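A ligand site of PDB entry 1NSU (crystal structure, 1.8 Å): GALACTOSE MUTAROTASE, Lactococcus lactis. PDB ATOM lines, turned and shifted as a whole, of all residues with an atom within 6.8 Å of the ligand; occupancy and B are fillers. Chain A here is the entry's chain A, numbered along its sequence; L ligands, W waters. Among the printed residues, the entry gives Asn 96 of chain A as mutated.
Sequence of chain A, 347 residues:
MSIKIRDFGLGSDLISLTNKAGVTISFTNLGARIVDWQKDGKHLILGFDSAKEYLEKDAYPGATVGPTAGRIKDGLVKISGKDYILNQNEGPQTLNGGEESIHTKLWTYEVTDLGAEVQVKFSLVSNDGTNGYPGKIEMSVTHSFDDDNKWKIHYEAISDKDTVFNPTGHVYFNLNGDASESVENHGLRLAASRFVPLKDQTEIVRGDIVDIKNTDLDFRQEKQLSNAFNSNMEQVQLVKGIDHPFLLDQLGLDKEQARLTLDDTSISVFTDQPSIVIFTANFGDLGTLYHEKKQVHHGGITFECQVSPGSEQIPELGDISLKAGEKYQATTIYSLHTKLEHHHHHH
The side-chain carboxylate (OD2) of Asp 243 sits at hydrogen-bond distance from an oxygen (O3) of the ligand (2.5 Å).
NE2 of His 170 is in hydrogen-bond range of O5 of the ligand, at 2.9 Å.
The side-chain carboxylate of Glu 304 is in hydrogen-bond range of an oxygen (O1) of the ligand.
The guanidinium group of Arg 71 sits at hydrogen-bond distance from an oxygen (O4) of the ligand (3.1 Å).
The backbone NH of Asn 96 sits at hydrogen-bond distance from the backbone carbonyl oxygen of Gly 70, at 2.8 Å.
NE of Arg 71 is in salt-bridge range of OE1 of Glu 90 (2.8 Å).
The side-chain carboxylate of Glu 304 is in hydrogen-bond range of the side-chain hydroxyl of Thr 302 (3.0 Å).
The backbone carbonyl oxygen of Glu 304 lies within hydrogen-bond range of the backbone NH of Val 277 (2.8 Å).
The backbone NH of Tyr 60 sits at hydrogen-bond distance from the side-chain carboxylate of Asp 58, 3.2 Å away.
The backbone NH (N) of Asp 243 sits close to the backbone carbonyl oxygen (O) of Ile 278 (3.3 Å).
The side-chain carboxylate of Glu 203 is in salt-bridge range of the guanidinium group of Arg 71, 3.8 Å away.
The backbone carbonyl oxygen (O) of Phe 279 lies within hydrogen-bond range of the backbone NH (N) of Thr 302, 3.0 Å away.
Tyr 60 touches the ligand (CD1 to C6, 3.6 Å).
Asn 96 touches the ligand.
OH of Tyr 172 touches O6 of the ligand, at 3.8 Å.
Glu 203 touches the ligand.
Phe 279 touches the ligand (CB to O1, 3.7 Å).
The nearest printed residue that does not touch the ligand is Leu 95 (4.3 Å).
Water W2 lies within hydrogen-bond range of the side-chain hydroxyl (OH) of Tyr 172 (2.6 Å), the side-chain carboxylate (OD2) of Asp 58 (2.7 Å) and an oxygen (O6) of the ligand (2.9 Å).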
ATOM      1  N   ASP A  58       0.086 -24.739 -20.720  1.00  0.00           N
ATOM      2  CA  ASP A  58       0.727 -23.503 -20.332  1.00  0.00           C
ATOM      3  C   ASP A  58       1.206 -22.888 -21.624  1.00  0.00           C
ATOM      4  O   ASP A  58       2.033 -23.510 -22.312  1.00  0.00           O
ATOM      5  CB  ASP A  58       1.918 -23.731 -19.387  1.00  0.00           C
ATOM      6  CG  ASP A  58       2.416 -22.424 -18.889  1.00  0.00           C
ATOM      7  OD1 ASP A  58       2.002 -21.365 -19.304  1.00  0.00           O
ATOM      8  OD2 ASP A  58       3.324 -22.529 -17.941  1.00  0.00           O
ATOM      9  N   TYR A  60       2.858 -20.053 -22.063  1.00  0.00           N
ATOM     10  CA  TYR A  60       4.015 -19.202 -22.021  1.00  0.00           C
ATOM     11  C   TYR A  60       5.355 -19.769 -22.369  1.00  0.00           C
ATOM     12  O   TYR A  60       6.183 -19.061 -22.971  1.00  0.00           O
ATOM     13  CB  TYR A  60       4.076 -18.582 -20.652  1.00  0.00           C
ATOM     14  CG  TYR A  60       3.008 -17.550 -20.432  1.00  0.00           C
ATOM     15  CD1 TYR A  60       2.223 -17.613 -19.291  1.00  0.00           C
ATOM     16  CD2 TYR A  60       2.802 -16.498 -21.323  1.00  0.00           C
ATOM     17  CE1 TYR A  60       1.246 -16.660 -19.017  1.00  0.00           C
ATOM     18  CE2 TYR A  60       1.838 -15.536 -21.063  1.00  0.00           C
ATOM     19  CZ  TYR A  60       1.053 -15.610 -19.912  1.00  0.00           C
ATOM     20  OH  TYR A  60       0.081 -14.673 -19.614  1.00  0.00           O
ATOM     21  N   PRO A  61       5.594 -21.047 -22.000  1.00  0.00           N
ATOM     22  CA  PRO A  61       6.896 -21.646 -22.251  1.00  0.00           C
ATOM     23  C   PRO A  61       7.474 -21.464 -23.649  1.00  0.00           C
ATOM     24  O   PRO A  61       6.857 -21.889 -24.622  1.00  0.00           O
ATOM     25  CB  PRO A  61       6.742 -23.140 -21.908  1.00  0.00           C
ATOM     26  CG  PRO A  61       5.546 -23.229 -20.997  1.00  0.00           C
ATOM     27  CD  PRO A  61       4.709 -22.000 -21.295  1.00  0.00           C
ATOM     28  N   GLY A  70       5.851  -9.176 -18.366  1.00  0.00           N
ATOM     29  CA  GLY A  70       5.751  -8.922 -16.955  1.00  0.00           C
ATOM     30  C   GLY A  70       4.407  -8.341 -16.521  1.00  0.00           C
ATOM     31  O   GLY A  70       3.441  -8.324 -17.304  1.00  0.00           O
ATOM     32  N   ARG A  71       4.383  -7.893 -15.247  1.00  0.00           N
ATOM     33  CA  ARG A  71       3.192  -7.335 -14.626  1.00  0.00           C
ATOM     34  C   ARG A  71       3.175  -5.855 -14.533  1.00  0.00           C
ATOM     35  O   ARG A  71       4.136  -5.239 -14.012  1.00  0.00           O
ATOM     36  CB  ARG A  71       3.004  -7.761 -13.175  1.00  0.00           C
ATOM     37  CG  ARG A  71       2.899  -9.258 -13.055  1.00  0.00           C
ATOM     38  CD  ARG A  71       2.972  -9.819 -11.655  1.00  0.00           C
ATOM     39  NE  ARG A  71       2.545 -11.227 -11.786  1.00  0.00           N
ATOM     40  CZ  ARG A  71       3.345 -12.253 -12.036  1.00  0.00           C
ATOM     41  NH1 ARG A  71       4.699 -12.113 -12.115  1.00  0.00           N
ATOM     42  NH2 ARG A  71       2.750 -13.461 -12.166  1.00  0.00           N
ATOM     43  N   GLU A  90      -4.770 -10.759 -14.548  1.00  0.00           N
ATOM     44  CA  GLU A  90      -4.289 -11.420 -13.359  1.00  0.00           C
ATOM     45  C   GLU A  90      -4.764 -10.536 -12.257  1.00  0.00           C
ATOM     46  O   GLU A  90      -4.008  -9.686 -11.815  1.00  0.00           O
ATOM     47  CB  GLU A  90      -2.758 -11.392 -13.352  1.00  0.00           C
ATOM     48  CG  GLU A  90      -2.292 -12.284 -12.211  1.00  0.00           C
ATOM     49  CD  GLU A  90      -0.798 -12.233 -12.003  1.00  0.00           C
ATOM     50  OE1 GLU A  90      -0.213 -11.212 -11.823  1.00  0.00           O
ATOM     51  OE2 GLU A  90      -0.226 -13.410 -12.019  1.00  0.00           O
ATOM     52  N   LEU A  95      -0.713  -8.907 -17.083  1.00  0.00           N
ATOM     53  CA  LEU A  95       0.468  -9.711 -17.060  1.00  0.00           C
ATOM     54  C   LEU A  95       0.796 -10.184 -18.454  1.00  0.00           C
ATOM     55  O   LEU A  95      -0.044 -10.703 -19.133  1.00  0.00           O
ATOM     56  CB  LEU A  95       0.227 -10.962 -16.160  1.00  0.00           C
ATOM     57  CG  LEU A  95       1.207 -12.106 -16.468  1.00  0.00           C
ATOM     58  CD1 LEU A  95       2.580 -11.887 -15.804  1.00  0.00           C
ATOM     59  CD2 LEU A  95       0.616 -13.409 -15.992  1.00  0.00           C
ATOM     60  N   ASN A  96       2.001 -10.041 -18.937  1.00  0.00           N
ATOM     61  CA  ASN A  96       2.293 -10.562 -20.276  1.00  0.00           C
ATOM     62  C   ASN A  96       1.392 -10.115 -21.454  1.00  0.00           C
ATOM     63  O   ASN A  96       1.094 -10.869 -22.397  1.00  0.00           O
ATOM     64  CB  ASN A  96       2.625 -12.060 -20.267  1.00  0.00           C
ATOM     65  CG  ASN A  96       3.797 -12.429 -19.361  1.00  0.00           C
ATOM     66  OD1 ASN A  96       4.687 -11.615 -19.110  1.00  0.00           O
ATOM     67  ND2 ASN A  96       3.811 -13.678 -18.882  1.00  0.00           N
ATOM     68  N   HIS A 170      10.345 -16.230 -23.443  1.00  0.00           N
ATOM     69  CA  HIS A 170      10.084 -16.922 -22.205  1.00  0.00           C
ATOM     70  C   HIS A 170      10.475 -18.410 -22.176  1.00  0.00           C
ATOM     71  O   HIS A 170       9.757 -19.242 -21.613  1.00  0.00           O
ATOM     72  CB  HIS A 170       8.565 -16.785 -21.973  1.00  0.00           C
ATOM     73  CG  HIS A 170       8.084 -16.827 -20.553  1.00  0.00           C
ATOM     74  ND1 HIS A 170       8.185 -17.992 -19.784  1.00  0.00           N
ATOM     75  CD2 HIS A 170       7.457 -15.875 -19.798  1.00  0.00           C
ATOM     76  CE1 HIS A 170       7.670 -17.674 -18.594  1.00  0.00           C
ATOM     77  NE2 HIS A 170       7.218 -16.424 -18.565  1.00  0.00           N
ATOM     78  N   TYR A 172      12.304 -21.777 -20.880  1.00  0.00           N
ATOM     79  CA  TYR A 172      12.696 -22.275 -19.571  1.00  0.00           C
ATOM     80  C   TYR A 172      13.800 -23.305 -19.848  1.00  0.00           C
ATOM     81  O   TYR A 172      13.651 -24.216 -20.668  1.00  0.00           O
ATOM     82  CB  TYR A 172      11.590 -23.075 -18.873  1.00  0.00           C
ATOM     83  CG  TYR A 172      10.438 -22.316 -18.231  1.00  0.00           C
ATOM     84  CD1 TYR A 172       9.277 -22.061 -18.951  1.00  0.00           C
ATOM     85  CD2 TYR A 172      10.482 -21.936 -16.888  1.00  0.00           C
ATOM     86  CE1 TYR A 172       8.194 -21.416 -18.366  1.00  0.00           C
ATOM     87  CE2 TYR A 172       9.424 -21.258 -16.285  1.00  0.00           C
ATOM     88  CZ  TYR A 172       8.267 -21.024 -17.032  1.00  0.00           C
ATOM     89  OH  TYR A 172       7.198 -20.381 -16.450  1.00  0.00           O
ATOM     90  N   GLU A 203       2.914  -9.906  -6.576  1.00  0.00           N
ATOM     91  CA  GLU A 203       4.076  -9.801  -7.432  1.00  0.00           C
ATOM     92  C   GLU A 203       4.298  -8.488  -8.118  1.00  0.00           C
ATOM     93  O   GLU A 203       5.071  -8.416  -9.044  1.00  0.00           O
ATOM     94  CB  GLU A 203       4.316 -11.020  -8.324  1.00  0.00           C
ATOM     95  CG  GLU A 203       4.383 -12.347  -7.529  1.00  0.00           C
ATOM     96  CD  GLU A 203       4.273 -13.642  -8.322  1.00  0.00           C
ATOM     97  OE1 GLU A 203       3.232 -14.291  -8.470  1.00  0.00           O
ATOM     98  OE2 GLU A 203       5.444 -14.046  -8.761  1.00  0.00           O
ATOM     99  N   ASP A 243      11.719 -14.993  -8.617  1.00  0.00           N
ATOM    100  CA  ASP A 243      10.735 -14.521  -9.577  1.00  0.00           C
ATOM    101  C   ASP A 243      10.947 -13.021  -9.554  1.00  0.00           C
ATOM    102  O   ASP A 243      10.112 -12.260  -9.113  1.00  0.00           O
ATOM    103  CB  ASP A 243       9.309 -14.903  -9.185  1.00  0.00           C
ATOM    104  CG  ASP A 243       8.401 -14.708 -10.372  1.00  0.00           C
ATOM    105  OD1 ASP A 243       8.768 -14.152 -11.391  1.00  0.00           O
ATOM    106  OD2 ASP A 243       7.204 -15.161 -10.208  1.00  0.00           O
ATOM    107  N   HIS A 244      12.150 -12.640 -10.001  1.00  0.00           N
ATOM    108  CA  HIS A 244      12.549 -11.257  -9.933  1.00  0.00           C
ATOM    109  C   HIS A 244      13.475 -10.741 -11.029  1.00  0.00           C
ATOM    110  O   HIS A 244      14.269 -11.497 -11.621  1.00  0.00           O
ATOM    111  CB  HIS A 244      13.491 -11.155  -8.694  1.00  0.00           C
ATOM    112  CG  HIS A 244      12.822 -11.455  -7.392  1.00  0.00           C
ATOM    113  ND1 HIS A 244      12.585 -12.758  -6.954  1.00  0.00           N
ATOM    114  CD2 HIS A 244      12.355 -10.563  -6.450  1.00  0.00           C
ATOM    115  CE1 HIS A 244      11.954 -12.649  -5.788  1.00  0.00           C
ATOM    116  NE2 HIS A 244      11.827 -11.343  -5.451  1.00  0.00           N
ATOM    117  N   VAL A 277      14.914 -10.955 -15.958  1.00  0.00           N
ATOM    118  CA  VAL A 277      13.956 -11.445 -15.019  1.00  0.00           C
ATOM    119  C   VAL A 277      14.163 -12.959 -14.864  1.00  0.00           C
ATOM    120  O   VAL A 277      14.110 -13.751 -15.836  1.00  0.00           O
ATOM    121  CB  VAL A 277      12.537 -11.139 -15.444  1.00  0.00           C
ATOM    122  CG1 VAL A 277      11.604 -11.927 -14.528  1.00  0.00           C
ATOM    123  CG2 VAL A 277      12.305  -9.634 -15.281  1.00  0.00           C
ATOM    124  N   ILE A 278      14.429 -13.400 -13.644  1.00  0.00           N
ATOM    125  CA  ILE A 278      14.662 -14.827 -13.449  1.00  0.00           C
ATOM    126  C   ILE A 278      13.538 -15.484 -12.685  1.00  0.00           C
ATOM    127  O   ILE A 278      13.246 -15.035 -11.572  1.00  0.00           O
ATOM    128  CB  ILE A 278      15.989 -15.063 -12.704  1.00  0.00           C
ATOM    129  CG1 ILE A 278      17.132 -14.722 -13.638  1.00  0.00           C
ATOM    130  CG2 ILE A 278      16.112 -16.544 -12.309  1.00  0.00           C
ATOM    131  CD1 ILE A 278      18.451 -14.602 -12.924  1.00  0.00           C
ATOM    132  N   PHE A 279      12.908 -16.507 -13.294  1.00  0.00           N
ATOM    133  CA  PHE A 279      11.809 -17.205 -12.629  1.00  0.00           C
ATOM    134  C   PHE A 279      12.094 -18.687 -12.641  1.00  0.00           C
ATOM    135  O   PHE A 279      12.300 -19.283 -13.706  1.00  0.00           O
ATOM    136  CB  PHE A 279      10.488 -16.900 -13.366  1.00  0.00           C
ATOM    137  CG  PHE A 279       9.275 -17.735 -12.976  1.00  0.00           C
ATOM    138  CD1 PHE A 279       8.723 -17.661 -11.691  1.00  0.00           C
ATOM    139  CD2 PHE A 279       8.661 -18.577 -13.904  1.00  0.00           C
ATOM    140  CE1 PHE A 279       7.599 -18.400 -11.335  1.00  0.00           C
ATOM    141  CE2 PHE A 279       7.548 -19.343 -13.572  1.00  0.00           C
ATOM    142  CZ  PHE A 279       7.001 -19.235 -12.290  1.00  0.00           C
ATOM    143  N   ASN A 282       8.366 -21.895  -9.875  1.00  0.00           N
ATOM    144  CA  ASN A 282       7.876 -22.104  -8.518  1.00  0.00           C
ATOM    145  C   ASN A 282       6.417 -22.541  -8.531  1.00  0.00           C
ATOM    146  O   ASN A 282       5.563 -21.865  -7.944  1.00  0.00           O
ATOM    147  CB  ASN A 282       8.008 -20.780  -7.745  1.00  0.00           C
ATOM    148  CG  ASN A 282       9.362 -20.152  -7.928  1.00  0.00           C
ATOM    149  OD1 ASN A 282      10.363 -20.855  -8.050  1.00  0.00           O
ATOM    150  ND2 ASN A 282       9.406 -18.812  -7.935  1.00  0.00           N
ATOM    151  N   PHE A 283       6.092 -23.653  -9.193  1.00  0.00           N
ATOM    152  CA  PHE A 283       4.699 -24.084  -9.293  1.00  0.00           C
ATOM    153  C   PHE A 283       4.195 -25.081  -8.262  1.00  0.00           C
ATOM    154  O   PHE A 283       3.088 -25.632  -8.408  1.00  0.00           O
ATOM    155  CB  PHE A 283       4.396 -24.675 -10.667  1.00  0.00           C
ATOM    156  CG  PHE A 283       4.762 -23.744 -11.806  1.00  0.00           C
ATOM    157  CD1 PHE A 283       5.815 -24.046 -12.675  1.00  0.00           C
ATOM    158  CD2 PHE A 283       4.000 -22.605 -12.074  1.00  0.00           C
ATOM    159  CE1 PHE A 283       6.111 -23.218 -13.767  1.00  0.00           C
ATOM    160  CE2 PHE A 283       4.288 -21.762 -13.148  1.00  0.00           C
ATOM    161  CZ  PHE A 283       5.349 -22.074 -13.985  1.00  0.00           C
ATOM    162  N   THR A 302      13.964 -19.395 -16.157  1.00  0.00           N
ATOM    163  CA  THR A 302      13.934 -18.496 -17.308  1.00  0.00           C
ATOM    164  C   THR A 302      15.011 -17.431 -17.232  1.00  0.00           C
ATOM    165  O   THR A 302      15.525 -17.143 -16.173  1.00  0.00           O
ATOM    166  CB  THR A 302      12.612 -17.664 -17.377  1.00  0.00           C
ATOM    167  OG1 THR A 302      12.629 -16.796 -16.261  1.00  0.00           O
ATOM    168  CG2 THR A 302      11.322 -18.464 -17.391  1.00  0.00           C
ATOM    169  N   GLU A 304      14.529 -13.916 -18.720  1.00  0.00           N
ATOM    170  CA  GLU A 304      13.739 -12.995 -19.518  1.00  0.00           C
ATOM    171  C   GLU A 304      14.424 -11.669 -19.644  1.00  0.00           C
ATOM    172  O   GLU A 304      14.385 -10.846 -18.727  1.00  0.00           O
ATOM    173  CB  GLU A 304      12.307 -12.871 -18.970  1.00  0.00           C
ATOM    174  CG  GLU A 304      11.612 -14.262 -18.868  1.00  0.00           C
ATOM    175  CD  GLU A 304      10.330 -14.235 -18.043  1.00  0.00           C
ATOM    176  OE1 GLU A 304       9.462 -13.420 -18.232  1.00  0.00           O
ATOM    177  OE2 GLU A 304      10.238 -15.147 -17.104  1.00  0.00           O
ATOM    178  N   PRO A 309      10.377  -4.998 -15.077  1.00  0.00           N
ATOM    179  CA  PRO A 309       8.996  -4.608 -14.879  1.00  0.00           C
ATOM    180  C   PRO A 309       8.952  -3.602 -13.744  1.00  0.00           C
ATOM    181  O   PRO A 309       9.910  -3.474 -12.995  1.00  0.00           O
ATOM    182  CB  PRO A 309       8.234  -5.892 -14.469  1.00  0.00           C
ATOM    183  CG  PRO A 309       9.196  -7.059 -14.669  1.00  0.00           C
ATOM    184  CD  PRO A 309      10.515  -6.486 -15.132  1.00  0.00           C
HETATM  185  C1  LIG L   1       6.757 -14.442 -15.584  1.00  0.00           C
HETATM  186  C2  LIG L   1       6.324 -14.203 -14.158  1.00  0.00           C
HETATM  187  C3  LIG L   1       6.172 -15.499 -13.420  1.00  0.00           C
HETATM  188  C4  LIG L   1       5.125 -16.285 -14.147  1.00  0.00           C
HETATM  189  C5  LIG L   1       5.494 -16.519 -15.619  1.00  0.00           C
HETATM  190  C6  LIG L   1       4.287 -17.062 -16.371  1.00  0.00           C
HETATM  191  O1  LIG L   1       8.021 -15.100 -15.485  1.00  0.00           O
HETATM  192  O2  LIG L   1       7.299 -13.440 -13.409  1.00  0.00           O
HETATM  193  O3  LIG L   1       5.642 -15.198 -12.114  1.00  0.00           O
HETATM  194  O4  LIG L   1       3.873 -15.645 -14.087  1.00  0.00           O
HETATM  195  O5  LIG L   1       5.790 -15.292 -16.305  1.00  0.00           O
HETATM  196  O6  LIG L   1       4.008 -18.387 -15.911  1.00  0.00           O
HETATM  197  O   HOH W   1       8.022 -10.708 -14.533  1.00  0.00           O
HETATM  198  O   HOH W   2       4.973 -20.398 -17.729  1.00  0.00           O
HETATM  199  O   HOH W   3       6.634 -13.292 -18.373  1.00  0.00           O
